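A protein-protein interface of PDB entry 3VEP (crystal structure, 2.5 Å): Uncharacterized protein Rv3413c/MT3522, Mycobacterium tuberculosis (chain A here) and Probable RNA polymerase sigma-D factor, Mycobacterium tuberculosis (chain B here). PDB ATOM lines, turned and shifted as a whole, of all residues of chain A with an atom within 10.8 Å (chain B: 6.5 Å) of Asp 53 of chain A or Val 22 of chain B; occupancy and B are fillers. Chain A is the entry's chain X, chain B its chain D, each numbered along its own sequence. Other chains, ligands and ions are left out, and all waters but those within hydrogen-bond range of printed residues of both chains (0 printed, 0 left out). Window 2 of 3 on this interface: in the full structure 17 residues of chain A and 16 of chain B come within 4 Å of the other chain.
The side-chain carboxylate (OD1) of Asp 53 of chain A sits close to the side-chain amide oxygen (OE1) of Gln 49 of chain A, at 2.7 Å.
The side-chain carboxylate (OD1) of Asp 20 of chain B lies close to the backbone NH (N) of Val 22 of chain B (3.2 Å).
The backbone carbonyl oxygen (O) of Val 22 of chain B lies close to the side-chain amide nitrogen (ND2) of Asn 26 of chain B, at 3.2 Å.
Among the printed residues, merely in contact across the chains: Leu 46 of chain A with Ser 21 of chain B, Leu 46 of chain A with Arg 24 of chain B, Leu 46 of chain A with Met 25 of chain B, Gln 49 of chain A with Ser 21 of chain B, Trp 50 of chain A with Val 22 of chain B, Trp 50 of chain A with Met 25 of chain B, Asp 53 of chain A with Ser 21 of chain B and Asp 53 of chain A with Val 22 of chain B.
Of the printed residues of chain B, Trp 50 of chain A touches Val 22 and Met 25.
No residue of chain A comes within 4 Å of Asp 20 of chain B.
Printed residues of chain A within 4 Å of Ser 21 of chain B: Leu 46, Gln 49 and Asp 53.
Of the printed residues of chain A, Val 22 of chain B touches Trp 50 and Asp 53.
No residue of chain A comes within 4 Å of Thr 23 of chain B.
Of the printed residues of chain A, Arg 24 of chain B touches Leu 46.
The nearest printed residue of chain A that does not touch Val 22 of chain B is Leu 54 of chain A (4.7 Å).
Of the 16 printed residues of chain A, 4 touch a printed residue of chain B.
Printed residues of chain A that touch a printed residue of chain B: Leu 46, Gln 49, Trp 50 and Asp 53.
Hydrophobic or aromatic side chains of chain A that line the printed part of chain B: Leu 46 and Trp 50.
Of the 9 printed residues of chain B, 4 touch a printed residue of chain A.
Among the printed residues, 8 pairs touch across the chains.
Among the printed residues, no Asp or Glu carboxylate lies within 4 Å of a Lys or Arg side-chain nitrogen of the other chain.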
ATOM      1  N   LEU A  27     -17.274  -5.318  -7.569  1.00  0.00           N
ATOM      2  CA  LEU A  27     -18.319  -5.386  -8.580  1.00  0.00           C
ATOM      3  C   LEU A  27     -18.962  -6.759  -8.564  1.00  0.00           C
ATOM      4  O   LEU A  27     -20.164  -6.879  -8.649  1.00  0.00           O
ATOM      5  CB  LEU A  27     -17.755  -5.087  -9.962  1.00  0.00           C
ATOM      6  CG  LEU A  27     -17.578  -3.563 -10.126  1.00  0.00           C
ATOM      7  CD1 LEU A  27     -16.770  -3.147 -11.369  1.00  0.00           C
ATOM      8  CD2 LEU A  27     -18.889  -2.788 -10.029  1.00  0.00           C
ATOM      9  N   ARG A  30     -21.313  -7.554  -5.914  1.00  0.00           N
ATOM     10  CA  ARG A  30     -22.337  -6.526  -5.863  1.00  0.00           C
ATOM     11  C   ARG A  30     -22.172  -5.518  -4.694  1.00  0.00           C
ATOM     12  O   ARG A  30     -23.115  -4.920  -4.232  1.00  0.00           O
ATOM     13  CB  ARG A  30     -23.723  -7.174  -5.917  1.00  0.00           C
ATOM     14  CG  ARG A  30     -23.936  -8.114  -7.124  1.00  0.00           C
ATOM     15  CD  ARG A  30     -25.420  -8.195  -7.555  1.00  0.00           C
ATOM     16  NE  ARG A  30     -26.226  -7.679  -6.471  1.00  0.00           N
ATOM     17  CZ  ARG A  30     -27.018  -6.626  -6.517  1.00  0.00           C
ATOM     18  NH1 ARG A  30     -27.212  -5.951  -7.638  1.00  0.00           N
ATOM     19  NH2 ARG A  30     -27.648  -6.283  -5.417  1.00  0.00           N
ATOM     20  N   ALA A  44     -18.573   2.306 -12.688  1.00  0.00           N
ATOM     21  CA  ALA A  44     -18.972   1.259 -11.759  1.00  0.00           C
ATOM     22  C   ALA A  44     -20.485   1.024 -11.814  1.00  0.00           C
ATOM     23  O   ALA A  44     -20.944  -0.120 -11.904  1.00  0.00           O
ATOM     24  CB  ALA A  44     -18.531   1.613 -10.342  1.00  0.00           C
ATOM     25  N   ALA A  45     -21.248   2.116 -11.778  1.00  0.00           N
ATOM     26  CA  ALA A  45     -22.706   2.061 -11.882  1.00  0.00           C
ATOM     27  C   ALA A  45     -23.122   1.362 -13.161  1.00  0.00           C
ATOM     28  O   ALA A  45     -23.956   0.448 -13.167  1.00  0.00           O
ATOM     29  CB  ALA A  45     -23.290   3.471 -11.855  1.00  0.00           C
ATOM     30  N   LEU A  46     -22.501   1.779 -14.250  1.00  0.00           N
ATOM     31  CA  LEU A  46     -22.795   1.212 -15.542  1.00  0.00           C
ATOM     32  C   LEU A  46     -22.517  -0.286 -15.599  1.00  0.00           C
ATOM     33  O   LEU A  46     -23.289  -1.044 -16.188  1.00  0.00           O
ATOM     34  CB  LEU A  46     -22.002   1.952 -16.593  1.00  0.00           C
ATOM     35  CG  LEU A  46     -22.259   1.478 -18.012  1.00  0.00           C
ATOM     36  CD1 LEU A  46     -23.746   1.554 -18.371  1.00  0.00           C
ATOM     37  CD2 LEU A  46     -21.380   2.268 -19.008  1.00  0.00           C
ATOM     38  N   LEU A  47     -21.432  -0.703 -14.955  1.00  0.00           N
ATOM     39  CA  LEU A  47     -21.044  -2.100 -14.927  1.00  0.00           C
ATOM     40  C   LEU A  47     -21.951  -2.908 -14.027  1.00  0.00           C
ATOM     41  O   LEU A  47     -22.286  -4.048 -14.330  1.00  0.00           O
ATOM     42  CB  LEU A  47     -19.605  -2.238 -14.444  1.00  0.00           C
ATOM     43  CG  LEU A  47     -18.540  -1.932 -15.498  1.00  0.00           C
ATOM     44  CD1 LEU A  47     -17.130  -1.681 -14.872  1.00  0.00           C
ATOM     45  CD2 LEU A  47     -18.506  -3.048 -16.525  1.00  0.00           C
ATOM     46  N   GLY A  48     -22.350  -2.314 -12.909  1.00  0.00           N
ATOM     47  CA  GLY A  48     -23.226  -3.015 -11.998  1.00  0.00           C
ATOM     48  C   GLY A  48     -24.562  -3.302 -12.666  1.00  0.00           C
ATOM     49  O   GLY A  48     -25.084  -4.437 -12.585  1.00  0.00           O
ATOM     50  N   GLN A  49     -25.122  -2.293 -13.343  1.00  0.00           N
ATOM     51  CA  GLN A  49     -26.427  -2.486 -13.971  1.00  0.00           C
ATOM     52  C   GLN A  49     -26.328  -3.590 -15.014  1.00  0.00           C
ATOM     53  O   GLN A  49     -27.222  -4.420 -15.169  1.00  0.00           O
ATOM     54  CB  GLN A  49     -26.970  -1.191 -14.580  1.00  0.00           C
ATOM     55  CG  GLN A  49     -28.409  -1.315 -15.067  1.00  0.00           C
ATOM     56  CD  GLN A  49     -29.340  -1.969 -14.020  1.00  0.00           C
ATOM     57  OE1 GLN A  49     -29.797  -3.119 -14.182  1.00  0.00           O
ATOM     58  NE2 GLN A  49     -29.613  -1.234 -12.938  1.00  0.00           N
ATOM     59  N   TRP A  50     -25.195  -3.604 -15.690  1.00  0.00           N
ATOM     60  CA  TRP A  50     -24.933  -4.514 -16.790  1.00  0.00           C
ATOM     61  C   TRP A  50     -24.733  -5.928 -16.273  1.00  0.00           C
ATOM     62  O   TRP A  50     -25.257  -6.880 -16.831  1.00  0.00           O
ATOM     63  CB  TRP A  50     -23.709  -3.992 -17.534  1.00  0.00           C
ATOM     64  CG  TRP A  50     -23.057  -4.922 -18.481  1.00  0.00           C
ATOM     65  CD1 TRP A  50     -23.471  -5.240 -19.748  1.00  0.00           C
ATOM     66  CD2 TRP A  50     -21.815  -5.608 -18.277  1.00  0.00           C
ATOM     67  NE1 TRP A  50     -22.565  -6.097 -20.335  1.00  0.00           N
ATOM     68  CE2 TRP A  50     -21.546  -6.347 -19.452  1.00  0.00           C
ATOM     69  CE3 TRP A  50     -20.915  -5.686 -17.208  1.00  0.00           C
ATOM     70  CZ2 TRP A  50     -20.414  -7.152 -19.588  1.00  0.00           C
ATOM     71  CZ3 TRP A  50     -19.786  -6.483 -17.346  1.00  0.00           C
ATOM     72  CH2 TRP A  50     -19.544  -7.203 -18.527  1.00  0.00           C
ATOM     73  N   ARG A  51     -23.968  -6.033 -15.195  1.00  0.00           N
ATOM     74  CA  ARG A  51     -23.803  -7.240 -14.405  1.00  0.00           C
ATOM     75  C   ARG A  51     -25.179  -7.795 -14.051  1.00  0.00           C
ATOM     76  O   ARG A  51     -25.469  -8.967 -14.294  1.00  0.00           O
ATOM     77  CB  ARG A  51     -23.037  -6.894 -13.107  1.00  0.00           C
ATOM     78  CG  ARG A  51     -22.828  -8.041 -12.093  1.00  0.00           C
ATOM     79  CD  ARG A  51     -22.627  -7.525 -10.653  1.00  0.00           C
ATOM     80  NE  ARG A  51     -23.662  -6.577 -10.251  1.00  0.00           N
ATOM     81  CZ  ARG A  51     -23.459  -5.463  -9.556  1.00  0.00           C
ATOM     82  NH1 ARG A  51     -22.247  -5.102  -9.153  1.00  0.00           N
ATOM     83  NH2 ARG A  51     -24.490  -4.681  -9.279  1.00  0.00           N
ATOM     84  N   ASP A  52     -26.027  -6.950 -13.478  1.00  0.00           N
ATOM     85  CA  ASP A  52     -27.368  -7.375 -13.094  1.00  0.00           C
ATOM     86  C   ASP A  52     -28.185  -7.927 -14.277  1.00  0.00           C
ATOM     87  O   ASP A  52     -28.623  -9.096 -14.242  1.00  0.00           O
ATOM     88  CB  ASP A  52     -28.100  -6.280 -12.294  1.00  0.00           C
ATOM     89  CG  ASP A  52     -27.524  -6.102 -10.866  1.00  0.00           C
ATOM     90  OD1 ASP A  52     -26.593  -6.835 -10.467  1.00  0.00           O
ATOM     91  OD2 ASP A  52     -28.008  -5.247 -10.107  1.00  0.00           O
ATOM     92  N   ASP A  53     -28.351  -7.117 -15.330  1.00  0.00           N
ATOM     93  CA  ASP A  53     -29.153  -7.510 -16.495  1.00  0.00           C
ATOM     94  C   ASP A  53     -28.708  -8.847 -17.050  1.00  0.00           C
ATOM     95  O   ASP A  53     -29.525  -9.691 -17.383  1.00  0.00           O
ATOM     96  CB  ASP A  53     -29.060  -6.475 -17.623  1.00  0.00           C
ATOM     97  CG  ASP A  53     -29.539  -5.089 -17.205  1.00  0.00           C
ATOM     98  OD1 ASP A  53     -30.204  -4.971 -16.142  1.00  0.00           O
ATOM     99  OD2 ASP A  53     -29.250  -4.121 -17.961  1.00  0.00           O
ATOM    100  N   LEU A  54     -27.403  -9.024 -17.160  1.00  0.00           N
ATOM    101  CA  LEU A  54     -26.827 -10.197 -17.777  1.00  0.00           C
ATOM    102  C   LEU A  54     -26.905 -11.429 -16.888  1.00  0.00           C
ATOM    103  O   LEU A  54     -26.792 -12.556 -17.374  1.00  0.00           O
ATOM    104  CB  LEU A  54     -25.363  -9.947 -18.139  1.00  0.00           C
ATOM    105  CG  LEU A  54     -24.997  -9.152 -19.395  1.00  0.00           C
ATOM    106  CD1 LEU A  54     -23.495  -9.336 -19.680  1.00  0.00           C
ATOM    107  CD2 LEU A  54     -25.813  -9.612 -20.583  1.00  0.00           C
ATOM    108  N   ARG A  55     -27.052 -11.215 -15.585  1.00  0.00           N
ATOM    109  CA  ARG A  55     -27.203 -12.328 -14.665  1.00  0.00           C
ATOM    110  C   ARG A  55     -28.671 -12.712 -14.694  1.00  0.00           C
ATOM    111  O   ARG A  55     -29.060 -13.862 -14.473  1.00  0.00           O
ATOM    112  CB  ARG A  55     -26.786 -11.913 -13.245  1.00  0.00           C
ATOM    113  CG  ARG A  55     -25.338 -12.239 -12.880  1.00  0.00           C
ATOM    114  CD  ARG A  55     -24.976 -11.547 -11.578  1.00  0.00           C
ATOM    115  NE  ARG A  55     -23.534 -11.469 -11.336  1.00  0.00           N
ATOM    116  CZ  ARG A  55     -22.985 -11.199 -10.146  1.00  0.00           C
ATOM    117  NH1 ARG A  55     -23.744 -10.986  -9.079  1.00  0.00           N
ATOM    118  NH2 ARG A  55     -21.675 -11.149 -10.016  1.00  0.00           N
ATOM    119  N   TRP A  56     -29.475 -11.707 -14.999  1.00  0.00           N
ATOM    120  CA  TRP A  56     -30.910 -11.765 -14.838  1.00  0.00           C
ATOM    121  C   TRP A  56     -31.560 -12.572 -15.944  1.00  0.00           C
ATOM    122  O   TRP A  56     -31.789 -12.068 -17.039  1.00  0.00           O
ATOM    123  CB  TRP A  56     -31.461 -10.351 -14.842  1.00  0.00           C
ATOM    124  CG  TRP A  56     -32.776 -10.240 -14.200  1.00  0.00           C
ATOM    125  CD1 TRP A  56     -33.903 -10.946 -14.515  1.00  0.00           C
ATOM    126  CD2 TRP A  56     -33.133  -9.370 -13.119  1.00  0.00           C
ATOM    127  NE1 TRP A  56     -34.939 -10.565 -13.700  1.00  0.00           N
ATOM    128  CE2 TRP A  56     -34.496  -9.597 -12.838  1.00  0.00           C
ATOM    129  CE3 TRP A  56     -32.436  -8.424 -12.368  1.00  0.00           C
ATOM    130  CZ2 TRP A  56     -35.173  -8.911 -11.824  1.00  0.00           C
ATOM    131  CZ3 TRP A  56     -33.108  -7.741 -11.361  1.00  0.00           C
ATOM    132  CH2 TRP A  56     -34.461  -7.987 -11.098  1.00  0.00           C
ATOM    133  N   PRO A  57     -31.907 -13.828 -15.634  1.00  0.00           N
ATOM    134  CA  PRO A  57     -32.388 -14.884 -16.557  1.00  0.00           C
ATOM    135  C   PRO A  57     -33.656 -14.508 -17.363  1.00  0.00           C
ATOM    136  O   PRO A  57     -33.570 -13.907 -18.425  1.00  0.00           O
ATOM    137  CB  PRO A  57     -32.729 -16.068 -15.623  1.00  0.00           C
ATOM    138  CG  PRO A  57     -32.387 -15.634 -14.251  1.00  0.00           C
ATOM    139  CD  PRO A  57     -31.984 -14.213 -14.214  1.00  0.00           C
ATOM    140  N   ALA B  19     -30.473   4.194 -24.803  1.00  0.00           N
ATOM    141  CA  ALA B  19     -29.991   2.808 -24.751  1.00  0.00           C
ATOM    142  C   ALA B  19     -29.901   2.281 -23.317  1.00  0.00           C
ATOM    143  O   ALA B  19     -29.536   3.016 -22.396  1.00  0.00           O
ATOM    144  CB  ALA B  19     -28.653   2.679 -25.446  1.00  0.00           C
ATOM    145  N   ASP B  20     -30.237   1.008 -23.122  1.00  0.00           N
ATOM    146  CA  ASP B  20     -30.123   0.403 -21.792  1.00  0.00           C
ATOM    147  C   ASP B  20     -28.653   0.090 -21.487  1.00  0.00           C
ATOM    148  O   ASP B  20     -27.789   0.181 -22.376  1.00  0.00           O
ATOM    149  CB  ASP B  20     -30.993  -0.860 -21.667  1.00  0.00           C
ATOM    150  CG  ASP B  20     -30.639  -1.924 -22.703  1.00  0.00           C
ATOM    151  OD1 ASP B  20     -29.477  -1.950 -23.158  1.00  0.00           O
ATOM    152  OD2 ASP B  20     -31.513  -2.737 -23.072  1.00  0.00           O
ATOM    153  N   SER B  21     -28.379  -0.285 -20.236  1.00  0.00           N
ATOM    154  CA  SER B  21     -27.009  -0.572 -19.813  1.00  0.00           C
ATOM    155  C   SER B  21     -26.320  -1.585 -20.724  1.00  0.00           C
ATOM    156  O   SER B  21     -25.144  -1.415 -21.068  1.00  0.00           O
ATOM    157  CB  SER B  21     -26.933  -0.997 -18.337  1.00  0.00           C
ATOM    158  OG  SER B  21     -26.660   0.129 -17.502  1.00  0.00           O
ATOM    159  N   VAL B  22     -27.053  -2.608 -21.156  1.00  0.00           N
ATOM    160  CA  VAL B  22     -26.424  -3.670 -21.938  1.00  0.00           C
ATOM    161  C   VAL B  22     -26.122  -3.284 -23.373  1.00  0.00           C
ATOM    162  O   VAL B  22     -25.042  -3.586 -23.877  1.00  0.00           O
ATOM    163  CB  VAL B  22     -27.102  -5.077 -21.781  1.00  0.00           C
ATOM    164  CG1 VAL B  22     -28.232  -5.105 -20.787  1.00  0.00           C
ATOM    165  CG2 VAL B  22     -27.248  -5.875 -23.081  1.00  0.00           C
ATOM    166  N   THR B  23     -27.061  -2.587 -24.005  1.00  0.00           N
ATOM    167  CA  THR B  23     -26.870  -2.056 -25.352  1.00  0.00           C
ATOM    168  C   THR B  23     -25.684  -1.117 -25.378  1.00  0.00           C
ATOM    169  O   THR B  23     -24.880  -1.116 -26.323  1.00  0.00           O
ATOM    170  CB  THR B  23     -28.111  -1.294 -25.828  1.00  0.00           C
ATOM    171  OG1 THR B  23     -28.972  -2.180 -26.564  1.00  0.00           O
ATOM    172  CG2 THR B  23     -27.704  -0.123 -26.739  1.00  0.00           C
ATOM    173  N   ARG B  24     -25.570  -0.328 -24.319  1.00  0.00           N
ATOM    174  CA  ARG B  24     -24.442   0.564 -24.166  1.00  0.00           C
ATOM    175  C   ARG B  24     -23.156  -0.157 -23.938  1.00  0.00           C
ATOM    176  O   ARG B  24     -22.211  -0.028 -24.706  1.00  0.00           O
ATOM    177  CB  ARG B  24     -24.661   1.386 -22.952  1.00  0.00           C
ATOM    178  CG  ARG B  24     -25.113   2.750 -23.176  1.00  0.00           C
ATOM    179  CD  ARG B  24     -25.384   3.117 -21.771  1.00  0.00           C
ATOM    180  NE  ARG B  24     -25.615   4.500 -21.496  1.00  0.00           N
ATOM    181  CZ  ARG B  24     -25.382   4.977 -20.286  1.00  0.00           C
ATOM    182  NH1 ARG B  24     -24.821   4.160 -19.403  1.00  0.00           N
ATOM    183  NH2 ARG B  24     -25.557   6.268 -19.989  1.00  0.00           N
ATOM    184  N   MET B  25     -23.125  -0.890 -22.836  1.00  0.00           N
ATOM    185  CA  MET B  25     -21.953  -1.661 -22.476  1.00  0.00           C
ATOM    186  C   MET B  25     -21.532  -2.546 -23.631  1.00  0.00           C
ATOM    187  O   MET B  25     -20.348  -2.667 -23.934  1.00  0.00           O
ATOM    188  CB  MET B  25     -22.238  -2.522 -21.252  1.00  0.00           C
ATOM    189  CG  MET B  25     -20.998  -3.117 -20.675  1.00  0.00           C
ATOM    190  SD  MET B  25     -19.791  -1.659 -20.215  1.00  0.00           S
ATOM    191  CE  MET B  25     -20.975  -0.802 -18.966  1.00  0.00           C
ATOM    192  N   ASN B  26     -22.513  -3.164 -24.272  1.00  0.00           N
ATOM    193  CA  ASN B  26     -22.241  -3.978 -25.439  1.00  0.00           C
ATOM    194  C   ASN B  26     -21.488  -3.188 -26.485  1.00  0.00           C
ATOM    195  O   ASN B  26     -20.458  -3.631 -27.002  1.00  0.00           O
ATOM    196  CB  ASN B  26     -23.542  -4.509 -26.025  1.00  0.00           C
ATOM    197  CG  ASN B  26     -23.817  -5.933 -25.610  1.00  0.00           C
ATOM    198  OD1 ASN B  26     -22.894  -6.682 -25.294  1.00  0.00           O
ATOM    199  ND2 ASN B  26     -25.091  -6.325 -25.624  1.00  0.00           N
ATOM    200  N   GLU B  27     -22.012  -2.008 -26.797  1.00  0.00           N
ATOM    201  CA  GLU B  27     -21.322  -1.105 -27.688  1.00  0.00           C
ATOM    202  C   GLU B  27     -19.869  -1.003 -27.276  1.00  0.00           C
ATOM    203  O   GLU B  27     -18.990  -1.299 -28.069  1.00  0.00           O
ATOM    204  CB  GLU B  27     -21.989   0.265 -27.687  1.00  0.00           C
ATOM    205  CG  GLU B  27     -21.196   1.320 -28.440  1.00  0.00           C
ATOM    206  CD  GLU B  27     -22.013   2.563 -28.753  1.00  0.00           C
ATOM    207  OE1 GLU B  27     -22.730   2.560 -29.771  1.00  0.00           O
ATOM    208  OE2 GLU B  27     -21.936   3.548 -27.989  1.00  0.00           O
